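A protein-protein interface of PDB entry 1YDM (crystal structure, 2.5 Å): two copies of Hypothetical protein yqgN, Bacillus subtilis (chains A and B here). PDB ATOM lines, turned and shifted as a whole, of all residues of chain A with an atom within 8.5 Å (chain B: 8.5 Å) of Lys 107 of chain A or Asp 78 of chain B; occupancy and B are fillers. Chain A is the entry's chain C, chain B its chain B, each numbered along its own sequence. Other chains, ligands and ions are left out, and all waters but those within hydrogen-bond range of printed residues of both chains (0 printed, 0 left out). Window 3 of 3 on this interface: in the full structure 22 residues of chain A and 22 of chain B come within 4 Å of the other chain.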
ATOM      1  N   LYS A  74      18.174 -20.465  28.904  1.00  0.00           N
ATOM      2  CA  LYS A  74      18.258 -20.984  27.554  1.00  0.00           C
ATOM      3  C   LYS A  74      19.603 -21.700  27.506  1.00  0.00           C
ATOM      4  O   LYS A  74      20.645 -21.073  27.351  1.00  0.00           O
ATOM      5  CB  LYS A  74      18.197 -19.847  26.532  1.00  0.00           C
ATOM      6  CG  LYS A  74      17.535 -20.267  25.212  1.00  0.00           C
ATOM      7  CD  LYS A  74      16.033 -20.556  25.384  1.00  0.00           C
ATOM      8  CE  LYS A  74      15.422 -21.259  24.156  1.00  0.00           C
ATOM      9  NZ  LYS A  74      15.593 -20.545  22.847  1.00  0.00           N
ATOM     10  N   CYS A  75      19.569 -23.019  27.672  1.00  0.00           N
ATOM     11  CA  CYS A  75      20.783 -23.817  27.677  1.00  0.00           C
ATOM     12  C   CYS A  75      21.302 -24.177  26.298  1.00  0.00           C
ATOM     13  O   CYS A  75      20.531 -24.409  25.369  1.00  0.00           O
ATOM     14  CB  CYS A  75      20.577 -25.105  28.476  1.00  0.00           C
ATOM     15  SG  CYS A  75      20.468 -24.864  30.252  1.00  0.00           S
ATOM     16  N   HIS A  76      22.628 -24.215  26.190  1.00  0.00           N
ATOM     17  CA  HIS A  76      23.318 -24.562  24.958  1.00  0.00           C
ATOM     18  C   HIS A  76      23.685 -26.042  25.022  1.00  0.00           C
ATOM     19  O   HIS A  76      24.555 -26.438  25.802  1.00  0.00           O
ATOM     20  CB  HIS A  76      24.600 -23.731  24.817  1.00  0.00           C
ATOM     21  CG  HIS A  76      24.358 -22.283  24.525  1.00  0.00           C
ATOM     22  ND1 HIS A  76      23.879 -21.838  23.313  1.00  0.00           N
ATOM     23  CD2 HIS A  76      24.503 -21.182  25.299  1.00  0.00           C
ATOM     24  CE1 HIS A  76      23.737 -20.525  23.352  1.00  0.00           C
ATOM     25  NE2 HIS A  76      24.108 -20.103  24.548  1.00  0.00           N
ATOM     26  N   PRO A  77      23.022 -26.884  24.213  1.00  0.00           N
ATOM     27  CA  PRO A  77      23.355 -28.312  24.250  1.00  0.00           C
ATOM     28  C   PRO A  77      24.781 -28.483  23.744  1.00  0.00           C
ATOM     29  O   PRO A  77      25.349 -29.576  23.775  1.00  0.00           O
ATOM     30  CB  PRO A  77      22.315 -28.930  23.321  1.00  0.00           C
ATOM     31  CG  PRO A  77      22.110 -27.854  22.302  1.00  0.00           C
ATOM     32  CD  PRO A  77      22.039 -26.599  23.152  1.00  0.00           C
ATOM     33  N   GLN A  83      22.415 -19.347  29.299  1.00  0.00           N
ATOM     34  CA  GLN A  83      22.097 -17.927  29.329  1.00  0.00           C
ATOM     35  C   GLN A  83      20.602 -17.694  29.507  1.00  0.00           C
ATOM     36  O   GLN A  83      19.778 -18.299  28.823  1.00  0.00           O
ATOM     37  CB  GLN A  83      22.597 -17.262  28.046  1.00  0.00           C
ATOM     38  CG  GLN A  83      22.296 -18.046  26.771  1.00  0.00           C
ATOM     39  CD  GLN A  83      22.703 -17.299  25.503  1.00  0.00           C
ATOM     40  OE1 GLN A  83      22.607 -17.835  24.398  1.00  0.00           O
ATOM     41  NE2 GLN A  83      23.152 -16.055  25.658  1.00  0.00           N
ATOM     42  N   PHE A  84      20.259 -16.809  30.436  1.00  0.00           N
ATOM     43  CA  PHE A  84      18.864 -16.489  30.734  1.00  0.00           C
ATOM     44  C   PHE A  84      18.287 -15.405  29.830  1.00  0.00           C
ATOM     45  O   PHE A  84      18.903 -14.356  29.623  1.00  0.00           O
ATOM     46  CB  PHE A  84      18.743 -16.051  32.188  1.00  0.00           C
ATOM     47  CG  PHE A  84      18.965 -17.158  33.165  1.00  0.00           C
ATOM     48  CD1 PHE A  84      17.895 -17.908  33.636  1.00  0.00           C
ATOM     49  CD2 PHE A  84      20.245 -17.468  33.602  1.00  0.00           C
ATOM     50  CE1 PHE A  84      18.097 -18.951  34.531  1.00  0.00           C
ATOM     51  CE2 PHE A  84      20.458 -18.507  34.497  1.00  0.00           C
ATOM     52  CZ  PHE A  84      19.382 -19.252  34.963  1.00  0.00           C
ATOM     53  N   ARG A  85      17.091 -15.657  29.309  1.00  0.00           N
ATOM     54  CA  ARG A  85      16.409 -14.714  28.427  1.00  0.00           C
ATOM     55  C   ARG A  85      15.123 -14.236  29.099  1.00  0.00           C
ATOM     56  O   ARG A  85      14.439 -15.012  29.757  1.00  0.00           O
ATOM     57  CB  ARG A  85      16.068 -15.407  27.113  1.00  0.00           C
ATOM     58  CG  ARG A  85      17.244 -16.089  26.435  1.00  0.00           C
ATOM     59  CD  ARG A  85      18.121 -15.084  25.717  1.00  0.00           C
ATOM     60  NE  ARG A  85      19.199 -15.723  24.967  1.00  0.00           N
ATOM     61  CZ  ARG A  85      19.018 -16.632  24.013  1.00  0.00           C
ATOM     62  NH1 ARG A  85      17.793 -17.025  23.683  1.00  0.00           N
ATOM     63  NH2 ARG A  85      20.067 -17.147  23.386  1.00  0.00           N
ATOM     64  N   THR A  86      14.794 -12.961  28.945  1.00  0.00           N
ATOM     65  CA  THR A  86      13.576 -12.435  29.552  1.00  0.00           C
ATOM     66  C   THR A  86      12.367 -13.212  29.035  1.00  0.00           C
ATOM     67  O   THR A  86      12.290 -13.530  27.850  1.00  0.00           O
ATOM     68  CB  THR A  86      13.389 -10.933  29.232  1.00  0.00           C
ATOM     69  OG1 THR A  86      12.141 -10.471  29.768  1.00  0.00           O
ATOM     70  CG2 THR A  86      13.398 -10.702  27.720  1.00  0.00           C
ATOM     71  N   TYR A  87      11.428 -13.526  29.925  1.00  0.00           N
ATOM     72  CA  TYR A  87      10.225 -14.268  29.536  1.00  0.00           C
ATOM     73  C   TYR A  87       8.966 -13.420  29.757  1.00  0.00           C
ATOM     74  O   TYR A  87       8.482 -13.306  30.880  1.00  0.00           O
ATOM     75  CB  TYR A  87      10.161 -15.574  30.345  1.00  0.00           C
ATOM     76  CG  TYR A  87       8.994 -16.483  30.026  1.00  0.00           C
ATOM     77  CD1 TYR A  87       8.434 -16.513  28.752  1.00  0.00           C
ATOM     78  CD2 TYR A  87       8.475 -17.344  30.991  1.00  0.00           C
ATOM     79  CE1 TYR A  87       7.391 -17.374  28.444  1.00  0.00           C
ATOM     80  CE2 TYR A  87       7.428 -18.212  30.695  1.00  0.00           C
ATOM     81  CZ  TYR A  87       6.894 -18.223  29.419  1.00  0.00           C
ATOM     82  OH  TYR A  87       5.876 -19.098  29.113  1.00  0.00           O
ATOM     83  N   GLN A  88       8.448 -12.832  28.678  1.00  0.00           N
ATOM     84  CA  GLN A  88       7.255 -11.970  28.733  1.00  0.00           C
ATOM     85  C   GLN A  88       6.010 -12.703  29.220  1.00  0.00           C
ATOM     86  O   GLN A  88       5.670 -13.752  28.673  1.00  0.00           O
ATOM     87  CB  GLN A  88       6.926 -11.388  27.350  1.00  0.00           C
ATOM     88  CG  GLN A  88       8.086 -10.760  26.596  1.00  0.00           C
ATOM     89  CD  GLN A  88       7.775 -10.573  25.100  1.00  0.00           C
ATOM     90  OE1 GLN A  88       8.685 -10.452  24.271  1.00  0.00           O
ATOM     91  NE2 GLN A  88       6.480 -10.542  24.758  1.00  0.00           N
ATOM     92  N   PRO A 103       8.222 -22.092  25.715  1.00  0.00           N
ATOM     93  CA  PRO A 103       8.256 -20.648  25.952  1.00  0.00           C
ATOM     94  C   PRO A 103       9.136 -19.980  24.912  1.00  0.00           C
ATOM     95  O   PRO A 103      10.326 -20.291  24.793  1.00  0.00           O
ATOM     96  CB  PRO A 103       8.825 -20.549  27.365  1.00  0.00           C
ATOM     97  CG  PRO A 103       9.739 -21.733  27.435  1.00  0.00           C
ATOM     98  CD  PRO A 103       8.888 -22.816  26.811  1.00  0.00           C
ATOM     99  N   VAL A 104       8.533 -19.069  24.158  1.00  0.00           N
ATOM    100  CA  VAL A 104       9.220 -18.353  23.094  1.00  0.00           C
ATOM    101  C   VAL A 104      10.052 -17.182  23.623  1.00  0.00           C
ATOM    102  O   VAL A 104      11.071 -16.802  23.026  1.00  0.00           O
ATOM    103  CB  VAL A 104       8.194 -17.831  22.069  1.00  0.00           C
ATOM    104  CG1 VAL A 104       7.172 -16.951  22.775  1.00  0.00           C
ATOM    105  CG2 VAL A 104       8.900 -17.066  20.950  1.00  0.00           C
ATOM    106  N   GLU A 106      11.247 -11.967  22.619  1.00  0.00           N
ATOM    107  CA  GLU A 106      12.422 -11.173  22.952  1.00  0.00           C
ATOM    108  C   GLU A 106      13.626 -12.040  23.301  1.00  0.00           C
ATOM    109  O   GLU A 106      14.289 -11.817  24.318  1.00  0.00           O
ATOM    110  CB  GLU A 106      12.118 -10.230  24.120  1.00  0.00           C
ATOM    111  CG  GLU A 106      11.274  -9.020  23.752  1.00  0.00           C
ATOM    112  CD  GLU A 106      10.854  -8.213  24.966  1.00  0.00           C
ATOM    113  OE1 GLU A 106      11.741  -7.812  25.750  1.00  0.00           O
ATOM    114  OE2 GLU A 106       9.639  -7.978  25.135  1.00  0.00           O
ATOM    115  N   LYS A 107      13.901 -13.032  22.458  1.00  0.00           N
ATOM    116  CA  LYS A 107      15.044 -13.914  22.671  1.00  0.00           C
ATOM    117  C   LYS A 107      16.301 -13.103  22.402  1.00  0.00           C
ATOM    118  O   LYS A 107      17.423 -13.573  22.601  1.00  0.00           O
ATOM    119  CB  LYS A 107      14.970 -15.123  21.731  1.00  0.00           C
ATOM    120  CG  LYS A 107      14.939 -14.791  20.248  1.00  0.00           C
ATOM    121  CD  LYS A 107      16.329 -14.595  19.668  1.00  0.00           C
ATOM    122  CE  LYS A 107      16.249 -14.406  18.162  1.00  0.00           C
ATOM    123  NZ  LYS A 107      17.587 -14.319  17.526  1.00  0.00           N
ATOM    124  N   THR A 108      16.088 -11.870  21.950  1.00  0.00           N
ATOM    125  CA  THR A 108      17.173 -10.943  21.652  1.00  0.00           C
ATOM    126  C   THR A 108      17.540 -10.214  22.942  1.00  0.00           C
ATOM    127  O   THR A 108      16.747 -10.172  23.886  1.00  0.00           O
ATOM    128  CB  THR A 108      16.744  -9.896  20.596  1.00  0.00           C
ATOM    129  OG1 THR A 108      16.058 -10.551  19.520  1.00  0.00           O
ATOM    130  CG2 THR A 108      17.966  -9.170  20.038  1.00  0.00           C
ATOM    131  N   LYS A 109      18.739  -9.643  22.979  1.00  0.00           N
ATOM    132  CA  LYS A 109      19.208  -8.919  24.155  1.00  0.00           C
ATOM    133  C   LYS A 109      19.130  -9.833  25.379  1.00  0.00           C
ATOM    134  O   LYS A 109      18.169  -9.786  26.152  1.00  0.00           O
ATOM    135  CB  LYS A 109      18.359  -7.659  24.371  1.00  0.00           C
ATOM    136  CG  LYS A 109      18.805  -6.791  25.541  1.00  0.00           C
ATOM    137  CD  LYS A 109      17.891  -5.588  25.724  1.00  0.00           C
ATOM    138  CE  LYS A 109      18.276  -4.787  26.957  1.00  0.00           C
ATOM    139  NZ  LYS A 109      18.207  -5.605  28.203  1.00  0.00           N
ATOM    140  N   GLU A 110      20.149 -10.676  25.538  1.00  0.00           N
ATOM    141  CA  GLU A 110      20.222 -11.614  26.654  1.00  0.00           C
ATOM    142  C   GLU A 110      20.274 -10.892  27.996  1.00  0.00           C
ATOM    143  O   GLU A 110      20.699  -9.741  28.088  1.00  0.00           O
ATOM    144  CB  GLU A 110      21.455 -12.516  26.508  1.00  0.00           C
ATOM    145  CG  GLU A 110      21.370 -13.537  25.374  1.00  0.00           C
ATOM    146  CD  GLU A 110      21.191 -12.909  23.992  1.00  0.00           C
ATOM    147  OE1 GLU A 110      22.115 -12.199  23.525  1.00  0.00           O
ATOM    148  OE2 GLU A 110      20.123 -13.130  23.374  1.00  0.00           O
ATOM    149  N   VAL A 111      19.834 -11.582  29.037  1.00  0.00           N
ATOM    150  CA  VAL A 111      19.824 -11.013  30.369  1.00  0.00           C
ATOM    151  C   VAL A 111      21.138 -11.336  31.071  1.00  0.00           C
ATOM    152  O   VAL A 111      21.398 -12.493  31.395  1.00  0.00           O
ATOM    153  CB  VAL A 111      18.668 -11.588  31.189  1.00  0.00           C
ATOM    154  CG1 VAL A 111      18.511 -10.811  32.473  1.00  0.00           C
ATOM    155  CG2 VAL A 111      17.392 -11.551  30.371  1.00  0.00           C
ATOM    156  N   CYS B  75      18.298 -30.471  19.923  1.00  0.00           N
ATOM    157  CA  CYS B  75      18.129 -29.240  19.156  1.00  0.00           C
ATOM    158  C   CYS B  75      18.669 -27.963  19.794  1.00  0.00           C
ATOM    159  O   CYS B  75      18.567 -27.769  21.003  1.00  0.00           O
ATOM    160  CB  CYS B  75      16.652 -29.063  18.857  1.00  0.00           C
ATOM    161  SG  CYS B  75      15.649 -29.802  20.143  1.00  0.00           S
ATOM    162  N   HIS B  76      19.214 -27.086  18.953  1.00  0.00           N
ATOM    163  CA  HIS B  76      19.793 -25.826  19.401  1.00  0.00           C
ATOM    164  C   HIS B  76      18.802 -24.676  19.484  1.00  0.00           C
ATOM    165  O   HIS B  76      17.827 -24.622  18.736  1.00  0.00           O
ATOM    166  CB  HIS B  76      20.933 -25.398  18.476  1.00  0.00           C
ATOM    167  CG  HIS B  76      21.996 -26.434  18.305  1.00  0.00           C
ATOM    168  ND1 HIS B  76      21.839 -27.532  17.486  1.00  0.00           N
ATOM    169  CD2 HIS B  76      23.233 -26.537  18.842  1.00  0.00           C
ATOM    170  CE1 HIS B  76      22.935 -28.266  17.526  1.00  0.00           C
ATOM    171  NE2 HIS B  76      23.797 -27.686  18.341  1.00  0.00           N
ATOM    172  N   PRO B  77      19.060 -23.724  20.396  1.00  0.00           N
ATOM    173  CA  PRO B  77      18.229 -22.539  20.626  1.00  0.00           C
ATOM    174  C   PRO B  77      18.494 -21.415  19.619  1.00  0.00           C
ATOM    175  O   PRO B  77      19.546 -21.384  18.972  1.00  0.00           O
ATOM    176  CB  PRO B  77      18.616 -22.130  22.041  1.00  0.00           C
ATOM    177  CG  PRO B  77      20.081 -22.428  22.053  1.00  0.00           C
ATOM    178  CD  PRO B  77      20.130 -23.805  21.410  1.00  0.00           C
ATOM    179  N   ASP B  78      17.530 -20.497  19.510  1.00  0.00           N
ATOM    180  CA  ASP B  78      17.601 -19.348  18.607  1.00  0.00           C
ATOM    181  C   ASP B  78      17.613 -19.765  17.138  1.00  0.00           C
ATOM    182  O   ASP B  78      17.508 -18.920  16.248  1.00  0.00           O
ATOM    183  CB  ASP B  78      18.843 -18.504  18.917  1.00  0.00           C
ATOM    184  CG  ASP B  78      18.820 -17.912  20.323  1.00  0.00           C
ATOM    185  OD1 ASP B  78      17.924 -17.092  20.622  1.00  0.00           O
ATOM    186  OD2 ASP B  78      19.704 -18.270  21.128  1.00  0.00           O
ATOM    187  N   THR B  79      17.743 -21.067  16.895  1.00  0.00           N
ATOM    188  CA  THR B  79      17.760 -21.625  15.544  1.00  0.00           C
ATOM    189  C   THR B  79      16.890 -22.866  15.471  1.00  0.00           C
ATOM    190  O   THR B  79      16.632 -23.515  16.488  1.00  0.00           O
ATOM    191  CB  THR B  79      19.178 -22.037  15.103  1.00  0.00           C
ATOM    192  OG1 THR B  79      19.101 -22.741  13.854  1.00  0.00           O
ATOM    193  CG2 THR B  79      19.818 -22.940  16.147  1.00  0.00           C
ATOM    194  N   LYS B  80      16.446 -23.204  14.266  1.00  0.00           N
ATOM    195  CA  LYS B  80      15.609 -24.383  14.081  1.00  0.00           C
ATOM    196  C   LYS B  80      16.461 -25.618  13.759  1.00  0.00           C
ATOM    197  O   LYS B  80      16.040 -26.501  13.011  1.00  0.00           O
ATOM    198  CB  LYS B  80      14.578 -24.121  12.973  1.00  0.00           C
ATOM    199  CG  LYS B  80      13.539 -23.054  13.334  1.00  0.00           C
ATOM    200  CD  LYS B  80      12.454 -22.918  12.266  1.00  0.00           C
ATOM    201  CE  LYS B  80      11.306 -22.029  12.736  1.00  0.00           C
ATOM    202  NZ  LYS B  80      11.753 -20.650  13.068  1.00  0.00           N
ATOM    203  N   LYS B  81      17.657 -25.671  14.341  1.00  0.00           N
ATOM    204  CA  LYS B  81      18.574 -26.782  14.130  1.00  0.00           C
ATOM    205  C   LYS B  81      18.381 -27.880  15.171  1.00  0.00           C
ATOM    206  O   LYS B  81      18.510 -27.647  16.375  1.00  0.00           O
ATOM    207  CB  LYS B  81      20.020 -26.284  14.177  1.00  0.00           C
ATOM    208  CG  LYS B  81      21.073 -27.373  14.025  1.00  0.00           C
ATOM    209  CD  LYS B  81      20.994 -28.066  12.667  1.00  0.00           C
ATOM    210  CE  LYS B  81      21.391 -27.137  11.530  1.00  0.00           C
ATOM    211  NZ  LYS B  81      21.343 -27.830  10.220  1.00  0.00           N
ATOM    212  N   GLY B 137       8.879 -24.537  18.673  1.00  0.00           N
ATOM    213  CA  GLY B 137      10.218 -24.406  18.128  1.00  0.00           C
ATOM    214  C   GLY B 137      10.227 -24.462  16.609  1.00  0.00           C
ATOM    215  O   GLY B 137      10.881 -23.655  15.950  1.00  0.00           O
ATOM    216  N   TYR B 139      11.179 -27.182  15.039  1.00  0.00           N
ATOM    217  CA  TYR B 139      12.297 -28.055  14.715  1.00  0.00           C
ATOM    218  C   TYR B 139      11.876 -29.200  13.818  1.00  0.00           C
ATOM    219  O   TYR B 139      12.563 -29.532  12.857  1.00  0.00           O
ATOM    220  CB  TYR B 139      12.918 -28.626  15.990  1.00  0.00           C
ATOM    221  CG  TYR B 139      13.474 -27.579  16.916  1.00  0.00           C
ATOM    222  CD1 TYR B 139      12.719 -27.081  17.976  1.00  0.00           C
ATOM    223  CD2 TYR B 139      14.761 -27.077  16.732  1.00  0.00           C
ATOM    224  CE1 TYR B 139      13.240 -26.104  18.835  1.00  0.00           C
ATOM    225  CE2 TYR B 139      15.285 -26.103  17.579  1.00  0.00           C
ATOM    226  CZ  TYR B 139      14.521 -25.627  18.625  1.00  0.00           C
ATOM    227  OH  TYR B 139      15.052 -24.680  19.464  1.00  0.00           O
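Printed residues of chain A that touch a printed residue of chain B: Lys 74, Cys 75, Pro 77, Arg 85 and Lys 107. Hydrophobic or aromatic side chains of chain A that line the printed part of chain B: Pro 77. Along chain A the printed residues that touch a printed residue of chain B span positions 74 to 107. Of the 9 printed residues of chain B, 4 touch a printed residue of chain A.
Among the printed residues, pairs that only touch across the chains: Lys 107 of chain A with Asp 78 of chain B, Lys 74 of chain A with Pro 77 of chain B, Pro 77 of chain A with Cys 75 of chain B, Pro 77 of chain A with Pro 77 of chain B, Lys 74 of chain A with Asp 78 of chain B, Pro 77 of chain A with His 76 of chain B and Cys 75 of chain A with Pro 77 of chain B.
NH2 of Arg 85 of chain A is in salt-bridge range of OD2 of Asp 78 of chain B (2.5 Å).
The side-chain carboxylate of Glu 110 of chain A lies within salt-bridge range of the guanidinium group of Arg 85 of chain A (3.2 Å). The backbone NH (N) of His 76 of chain B lies within hydrogen-bond range of the backbone carbonyl oxygen (O) of Lys 81 of chain B, 2.7 Å away. OE1 of Gln 83 of chain A lies within hydrogen-bond range of NH2 of Arg 85 of chain A, at 2.8 Å. O of Gln 83 of chain A sits at hydrogen-bond distance from N of Lys 74 of chain A (2.7 Å). The side-chain hydroxyl (OH) of Tyr 139 of chain B lies within hydrogen-bond range of the backbone carbonyl oxygen (O) of His 76 of chain B (2.9 Å).
Cys 75 of chain A touches Pro 77 of chain B, and with the chains exchanged Pro 77 of chain A touches Cys 75 of chain B. Pro 77 of chain A touches His 76 of chain B, but with the chains exchanged His 76 of chain A does not touch Pro 77 of chain B (4.04 Å). Pro 77 of chain A touches its own counterpart, Pro 77 of chain B. Of the 8 pairs that touch across the chains among the printed residues, 3 have their exchanged pair printed and touching as well.
Of the printed residues of chain B, Cys 75 of chain A touches Pro 77 (3.9 Å). Of the printed residues of chain B, Pro 77 of chain A touches Cys 75, His 76 and Pro 77. Glu 106 of chain A touches none of the printed residues of chain B. Of the printed residues of chain B, Lys 107 of chain A touches Asp 78. Of the printed residues of chain A, Cys 75 of chain B touches Pro 77 (3.8 Å). Of the printed residues of chain A, His 76 of chain B touches Pro 77 (3.9 Å). Printed residues of chain A within 4 Å of Pro 77 of chain B: Lys 74, Cys 75 and Pro 77. Printed residues of chain A within 4 Å of Asp 78 of chain B: Lys 74 (3.9 Å), Arg 85 (2.5 Å) and Lys 107 (3.1 Å). The nearest residue of chain B that does not touch Lys 107 of chain A is Thr 79 of chain B (6.8 Å). The nearest residue of chain A that does not touch Asp 78 of chain B is Gln 83 of chain A (4.4 Å).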
